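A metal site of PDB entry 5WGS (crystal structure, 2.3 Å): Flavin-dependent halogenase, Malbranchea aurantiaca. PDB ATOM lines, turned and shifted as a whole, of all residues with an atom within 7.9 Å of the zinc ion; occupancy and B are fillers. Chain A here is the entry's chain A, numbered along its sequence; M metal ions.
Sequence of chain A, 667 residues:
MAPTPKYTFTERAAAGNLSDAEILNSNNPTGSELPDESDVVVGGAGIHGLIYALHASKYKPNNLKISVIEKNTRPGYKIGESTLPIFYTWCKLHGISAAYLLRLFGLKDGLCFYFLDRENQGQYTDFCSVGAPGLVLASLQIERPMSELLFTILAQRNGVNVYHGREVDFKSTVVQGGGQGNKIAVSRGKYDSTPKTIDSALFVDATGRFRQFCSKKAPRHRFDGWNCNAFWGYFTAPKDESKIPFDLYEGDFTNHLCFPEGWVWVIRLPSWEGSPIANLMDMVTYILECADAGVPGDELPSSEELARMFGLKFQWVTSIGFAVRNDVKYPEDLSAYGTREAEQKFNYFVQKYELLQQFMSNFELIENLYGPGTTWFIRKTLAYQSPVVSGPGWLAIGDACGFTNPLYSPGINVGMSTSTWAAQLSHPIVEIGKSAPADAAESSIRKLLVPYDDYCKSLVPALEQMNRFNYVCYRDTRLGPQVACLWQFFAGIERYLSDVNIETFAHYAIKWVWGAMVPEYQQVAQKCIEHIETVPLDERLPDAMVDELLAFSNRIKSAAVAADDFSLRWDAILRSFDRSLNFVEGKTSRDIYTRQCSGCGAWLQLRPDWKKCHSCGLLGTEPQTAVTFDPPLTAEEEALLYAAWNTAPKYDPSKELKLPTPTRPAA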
ATOM      1  N   SER A 302     -27.644   9.588  16.874  1.00  0.00           N
ATOM      2  CA  SER A 302     -26.669   9.709  17.943  1.00  0.00           C
ATOM      3  C   SER A 302     -26.447  11.175  18.294  1.00  0.00           C
ATOM      4  O   SER A 302     -26.835  12.077  17.551  1.00  0.00           O
ATOM      5  CB  SER A 302     -25.342   9.054  17.548  1.00  0.00           C
ATOM      6  OG  SER A 302     -24.674   9.785  16.531  1.00  0.00           O
ATOM      7  N   GLU A 304     -23.752  13.041  18.284  1.00  0.00           N
ATOM      8  CA  GLU A 304     -23.011  13.794  17.275  1.00  0.00           C
ATOM      9  C   GLU A 304     -23.839  14.015  16.016  1.00  0.00           C
ATOM     10  O   GLU A 304     -23.687  15.036  15.355  1.00  0.00           O
ATOM     11  CB  GLU A 304     -21.696  13.084  16.947  1.00  0.00           C
ATOM     12  CG  GLU A 304     -20.675  13.116  18.094  1.00  0.00           C
ATOM     13  CD  GLU A 304     -19.449  12.254  17.811  1.00  0.00           C
ATOM     14  OE1 GLU A 304     -19.141  11.998  16.621  1.00  0.00           O
ATOM     15  OE2 GLU A 304     -18.804  11.825  18.797  1.00  0.00           O
ATOM     16  N   TRP A 316     -16.897  16.273  24.856  1.00  0.00           N
ATOM     17  CA  TRP A 316     -16.807  15.604  26.143  1.00  0.00           C
ATOM     18  C   TRP A 316     -15.861  16.367  27.051  1.00  0.00           C
ATOM     19  O   TRP A 316     -14.742  16.710  26.648  1.00  0.00           O
ATOM     20  CB  TRP A 316     -16.329  14.158  25.962  1.00  0.00           C
ATOM     21  CG  TRP A 316     -17.387  13.272  25.425  1.00  0.00           C
ATOM     22  CD1 TRP A 316     -17.554  12.894  24.117  1.00  0.00           C
ATOM     23  CD2 TRP A 316     -18.452  12.663  26.155  1.00  0.00           C
ATOM     24  NE1 TRP A 316     -18.655  12.080  24.011  1.00  0.00           N
ATOM     25  CE2 TRP A 316     -19.224  11.923  25.243  1.00  0.00           C
ATOM     26  CE3 TRP A 316     -18.827  12.669  27.504  1.00  0.00           C
ATOM     27  CZ2 TRP A 316     -20.343  11.187  25.637  1.00  0.00           C
ATOM     28  CZ3 TRP A 316     -19.943  11.945  27.895  1.00  0.00           C
ATOM     29  CH2 TRP A 316     -20.691  11.216  26.958  1.00  0.00           C
ATOM     30  N   ARG A 595     -19.784  -0.555  28.778  1.00  0.00           N
ATOM     31  CA  ARG A 595     -18.564  -0.632  27.988  1.00  0.00           C
ATOM     32  C   ARG A 595     -18.249   0.745  27.432  1.00  0.00           C
ATOM     33  O   ARG A 595     -19.142   1.581  27.273  1.00  0.00           O
ATOM     34  CB  ARG A 595     -18.686  -1.645  26.827  1.00  0.00           C
ATOM     35  CG  ARG A 595     -19.490  -1.147  25.644  1.00  0.00           C
ATOM     36  CD  ARG A 595     -19.403  -2.085  24.454  1.00  0.00           C
ATOM     37  NE  ARG A 595     -20.281  -1.664  23.359  1.00  0.00           N
ATOM     38  CZ  ARG A 595     -19.887  -0.968  22.296  1.00  0.00           C
ATOM     39  NH1 ARG A 595     -18.615  -0.614  22.163  1.00  0.00           N
ATOM     40  NH2 ARG A 595     -20.774  -0.632  21.357  1.00  0.00           N
ATOM     41  N   GLN A 596     -16.976   0.989  27.139  1.00  0.00           N
ATOM     42  CA  GLN A 596     -16.534   2.246  26.536  1.00  0.00           C
ATOM     43  C   GLN A 596     -16.504   2.094  25.019  1.00  0.00           C
ATOM     44  O   GLN A 596     -15.988   1.099  24.501  1.00  0.00           O
ATOM     45  CB  GLN A 596     -15.151   2.641  27.064  1.00  0.00           C
ATOM     46  CG  GLN A 596     -14.923   4.142  27.179  1.00  0.00           C
ATOM     47  CD  GLN A 596     -13.517   4.488  27.685  1.00  0.00           C
ATOM     48  OE1 GLN A 596     -12.694   3.598  27.915  1.00  0.00           O
ATOM     49  NE2 GLN A 596     -13.253   5.781  27.846  1.00  0.00           N
ATOM     50  N   CYS A 597     -17.068   3.071  24.308  1.00  0.00           N
ATOM     51  CA  CYS A 597     -16.989   3.043  22.850  1.00  0.00           C
ATOM     52  C   CYS A 597     -15.534   3.137  22.419  1.00  0.00           C
ATOM     53  O   CYS A 597     -14.778   3.963  22.930  1.00  0.00           O
ATOM     54  CB  CYS A 597     -17.774   4.195  22.223  1.00  0.00           C
ATOM     55  SG  CYS A 597     -17.803   4.119  20.394  1.00  0.00           S
ATOM     56  N   SER A 598     -15.136   2.258  21.492  1.00  0.00           N
ATOM     57  CA  SER A 598     -13.764   2.292  21.012  1.00  0.00           C
ATOM     58  C   SER A 598     -13.485   3.523  20.153  1.00  0.00           C
ATOM     59  O   SER A 598     -12.319   3.919  20.021  1.00  0.00           O
ATOM     60  CB  SER A 598     -13.466   1.009  20.223  1.00  0.00           C
ATOM     61  OG  SER A 598     -14.650   0.520  19.614  1.00  0.00           O
ATOM     62  N   GLY A 599     -14.529   4.151  19.605  1.00  0.00           N
ATOM     63  CA  GLY A 599     -14.372   5.261  18.684  1.00  0.00           C
ATOM     64  C   GLY A 599     -14.351   6.641  19.314  1.00  0.00           C
ATOM     65  O   GLY A 599     -13.486   7.457  18.979  1.00  0.00           O
ATOM     66  N   CYS A 600     -15.285   6.926  20.221  1.00  0.00           N
ATOM     67  CA  CYS A 600     -15.378   8.236  20.848  1.00  0.00           C
ATOM     68  C   CYS A 600     -15.114   8.233  22.340  1.00  0.00           C
ATOM     69  O   CYS A 600     -15.169   9.293  22.972  1.00  0.00           O
ATOM     70  CB  CYS A 600     -16.757   8.851  20.586  1.00  0.00           C
ATOM     71  SG  CYS A 600     -18.105   7.910  21.362  1.00  0.00           S
ATOM     72  N   GLY A 601     -14.858   7.071  22.942  1.00  0.00           N
ATOM     73  CA  GLY A 601     -14.594   7.019  24.363  1.00  0.00           C
ATOM     74  C   GLY A 601     -15.798   7.172  25.256  1.00  0.00           C
ATOM     75  O   GLY A 601     -15.646   7.195  26.485  1.00  0.00           O
ATOM     76  N   ALA A 602     -16.998   7.286  24.692  1.00  0.00           N
ATOM     77  CA  ALA A 602     -18.202   7.423  25.496  1.00  0.00           C
ATOM     78  C   ALA A 602     -18.585   6.084  26.103  1.00  0.00           C
ATOM     79  O   ALA A 602     -18.332   5.013  25.536  1.00  0.00           O
ATOM     80  CB  ALA A 602     -19.354   7.958  24.661  1.00  0.00           C
ATOM     81  N   TRP A 603     -19.205   6.157  27.275  1.00  0.00           N
ATOM     82  CA  TRP A 603     -19.616   4.948  27.977  1.00  0.00           C
ATOM     83  C   TRP A 603     -21.042   4.562  27.586  1.00  0.00           C
ATOM     84  O   TRP A 603     -21.915   5.421  27.420  1.00  0.00           O
ATOM     85  CB  TRP A 603     -19.489   5.146  29.477  1.00  0.00           C
ATOM     86  CG  TRP A 603     -18.050   5.149  29.938  1.00  0.00           C
ATOM     87  CD1 TRP A 603     -17.237   6.227  30.062  1.00  0.00           C
ATOM     88  CD2 TRP A 603     -17.279   4.007  30.336  1.00  0.00           C
ATOM     89  NE1 TRP A 603     -15.993   5.848  30.520  1.00  0.00           N
ATOM     90  CE2 TRP A 603     -15.997   4.490  30.699  1.00  0.00           C
ATOM     91  CE3 TRP A 603     -17.544   2.639  30.431  1.00  0.00           C
ATOM     92  CZ2 TRP A 603     -14.980   3.636  31.138  1.00  0.00           C
ATOM     93  CZ3 TRP A 603     -16.533   1.794  30.869  1.00  0.00           C
ATOM     94  CH2 TRP A 603     -15.268   2.299  31.217  1.00  0.00           C
ATOM     95  N   LEU A 604     -21.273   3.256  27.435  1.00  0.00           N
ATOM     96  CA  LEU A 604     -22.495   2.726  26.861  1.00  0.00           C
ATOM     97  C   LEU A 604     -23.107   1.694  27.790  1.00  0.00           C
ATOM     98  O   LEU A 604     -22.403   0.970  28.509  1.00  0.00           O
ATOM     99  CB  LEU A 604     -22.226   2.095  25.496  1.00  0.00           C
ATOM    100  CG  LEU A 604     -21.444   2.974  24.524  1.00  0.00           C
ATOM    101  CD1 LEU A 604     -21.104   2.204  23.267  1.00  0.00           C
ATOM    102  CD2 LEU A 604     -22.247   4.236  24.182  1.00  0.00           C
ATOM    103  N   LYS A 612     -25.546   0.044  18.568  1.00  0.00           N
ATOM    104  CA  LYS A 612     -24.706   1.167  18.173  1.00  0.00           C
ATOM    105  C   LYS A 612     -24.481   2.095  19.364  1.00  0.00           C
ATOM    106  O   LYS A 612     -25.287   2.167  20.298  1.00  0.00           O
ATOM    107  CB  LYS A 612     -25.352   1.957  17.018  1.00  0.00           C
ATOM    108  CG  LYS A 612     -26.372   2.990  17.487  1.00  0.00           C
ATOM    109  CD  LYS A 612     -26.897   3.847  16.355  1.00  0.00           C
ATOM    110  CE  LYS A 612     -27.825   4.945  16.872  1.00  0.00           C
ATOM    111  NZ  LYS A 612     -28.546   5.637  15.758  1.00  0.00           N
ATOM    112  N   CYS A 613     -23.352   2.814  19.314  1.00  0.00           N
ATOM    113  CA  CYS A 613     -23.095   3.874  20.265  1.00  0.00           C
ATOM    114  C   CYS A 613     -24.134   4.988  20.107  1.00  0.00           C
ATOM    115  O   CYS A 613     -24.365   5.483  19.000  1.00  0.00           O
ATOM    116  CB  CYS A 613     -21.680   4.422  20.061  1.00  0.00           C
ATOM    117  SG  CYS A 613     -21.192   5.819  21.114  1.00  0.00           S
ATOM    118  N   HIS A 614     -24.793   5.345  21.206  1.00  0.00           N
ATOM    119  CA  HIS A 614     -25.795   6.411  21.189  1.00  0.00           C
ATOM    120  C   HIS A 614     -25.191   7.793  21.067  1.00  0.00           C
ATOM    121  O   HIS A 614     -25.937   8.769  20.922  1.00  0.00           O
ATOM    122  CB  HIS A 614     -26.630   6.348  22.468  1.00  0.00           C
ATOM    123  CG  HIS A 614     -25.829   6.558  23.710  1.00  0.00           C
ATOM    124  ND1 HIS A 614     -25.517   7.819  24.193  1.00  0.00           N
ATOM    125  CD2 HIS A 614     -25.241   5.680  24.561  1.00  0.00           C
ATOM    126  CE1 HIS A 614     -24.787   7.698  25.283  1.00  0.00           C
ATOM    127  NE2 HIS A 614     -24.602   6.408  25.530  1.00  0.00           N
ATOM    128  N   SER A 615     -23.856   7.911  21.128  1.00  0.00           N
ATOM    129  CA  SER A 615     -23.163   9.185  21.167  1.00  0.00           C
ATOM    130  C   SER A 615     -22.523   9.547  19.837  1.00  0.00           C
ATOM    131  O   SER A 615     -22.671  10.679  19.366  1.00  0.00           O
ATOM    132  CB  SER A 615     -22.094   9.157  22.272  1.00  0.00           C
ATOM    133  OG  SER A 615     -21.539  10.437  22.489  1.00  0.00           O
ATOM    134  N   CYS A 616     -21.815   8.603  19.214  1.00  0.00           N
ATOM    135  CA  CYS A 616     -21.204   8.821  17.911  1.00  0.00           C
ATOM    136  C   CYS A 616     -21.844   7.975  16.804  1.00  0.00           C
ATOM    137  O   CYS A 616     -21.588   8.245  15.618  1.00  0.00           O
ATOM    138  CB  CYS A 616     -19.695   8.546  17.955  1.00  0.00           C
ATOM    139  SG  CYS A 616     -19.185   6.803  17.935  1.00  0.00           S
ATOM    140  N   GLY A 617     -22.666   6.984  17.145  1.00  0.00           N
ATOM    141  CA  GLY A 617     -23.311   6.155  16.159  1.00  0.00           C
ATOM    142  C   GLY A 617     -22.501   4.958  15.699  1.00  0.00           C
ATOM    143  O   GLY A 617     -23.014   4.152  14.922  1.00  0.00           O
ATOM    144  N   LEU A 618     -21.257   4.838  16.137  1.00  0.00           N
ATOM    145  CA  LEU A 618     -20.417   3.724  15.706  1.00  0.00           C
ATOM    146  C   LEU A 618     -21.016   2.393  16.167  1.00  0.00           C
ATOM    147  O   LEU A 618     -21.257   2.180  17.359  1.00  0.00           O
ATOM    148  CB  LEU A 618     -19.001   3.880  16.246  1.00  0.00           C
ATOM    149  CG  LEU A 618     -18.044   2.690  16.121  1.00  0.00           C
ATOM    150  CD1 LEU A 618     -17.817   2.336  14.653  1.00  0.00           C
ATOM    151  CD2 LEU A 618     -16.727   3.004  16.819  1.00  0.00           C
ATOM    152  N   LEU A 619     -21.230   1.500  15.204  1.00  0.00           N
ATOM    153  CA  LEU A 619     -21.786   0.192  15.510  1.00  0.00           C
ATOM    154  C   LEU A 619     -20.715  -0.705  16.120  1.00  0.00           C
ATOM    155  O   LEU A 619     -19.606  -0.829  15.591  1.00  0.00           O
ATOM    156  CB  LEU A 619     -22.342  -0.421  14.226  1.00  0.00           C
ATOM    157  CG  LEU A 619     -23.163  -1.702  14.326  1.00  0.00           C
ATOM    158  CD1 LEU A 619     -24.474  -1.510  13.579  1.00  0.00           C
ATOM    159  CD2 LEU A 619     -22.386  -2.866  13.759  1.00  0.00           C
HETATM  160 ZN    ZN M   1     -19.073   6.246  20.122  1.00  0.00          ZN
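The backbone NH of Leu 618 lies close to the side-chain sulfur of Cys 616, 3.4 Å away.
The side-chain sulfur (SG) of Cys 600 lies close to the backbone NH (N) of Ala 602, at 3.6 Å.
The backbone NH (N) of Cys 613 lies within hydrogen-bond range of the backbone carbonyl oxygen (O) of Leu 618, at 2.9 Å.
The backbone NH of Ser 615 sits close to the side-chain sulfur of Cys 613, 3.4 Å away.
The side-chain sulfur (SG) of Cys 597 sits close to the backbone NH (N) of Gly 599.
The backbone carbonyl oxygen (O) of Ala 602 sits at hydrogen-bond distance from the backbone NH (N) of Cys 597.
Along chain A the residues within 4 Å of the zinc ion span positions 597 to 616.
The zinc ion is bound by the side-chain sulfur (SG) of Cys 616, the side-chain sulfur (SG) of Cys 600, the side-chain sulfur (SG) of Cys 613 and the side-chain sulfur (SG) of Cys 597.
The zinc ion has four donor atoms within binding distance.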
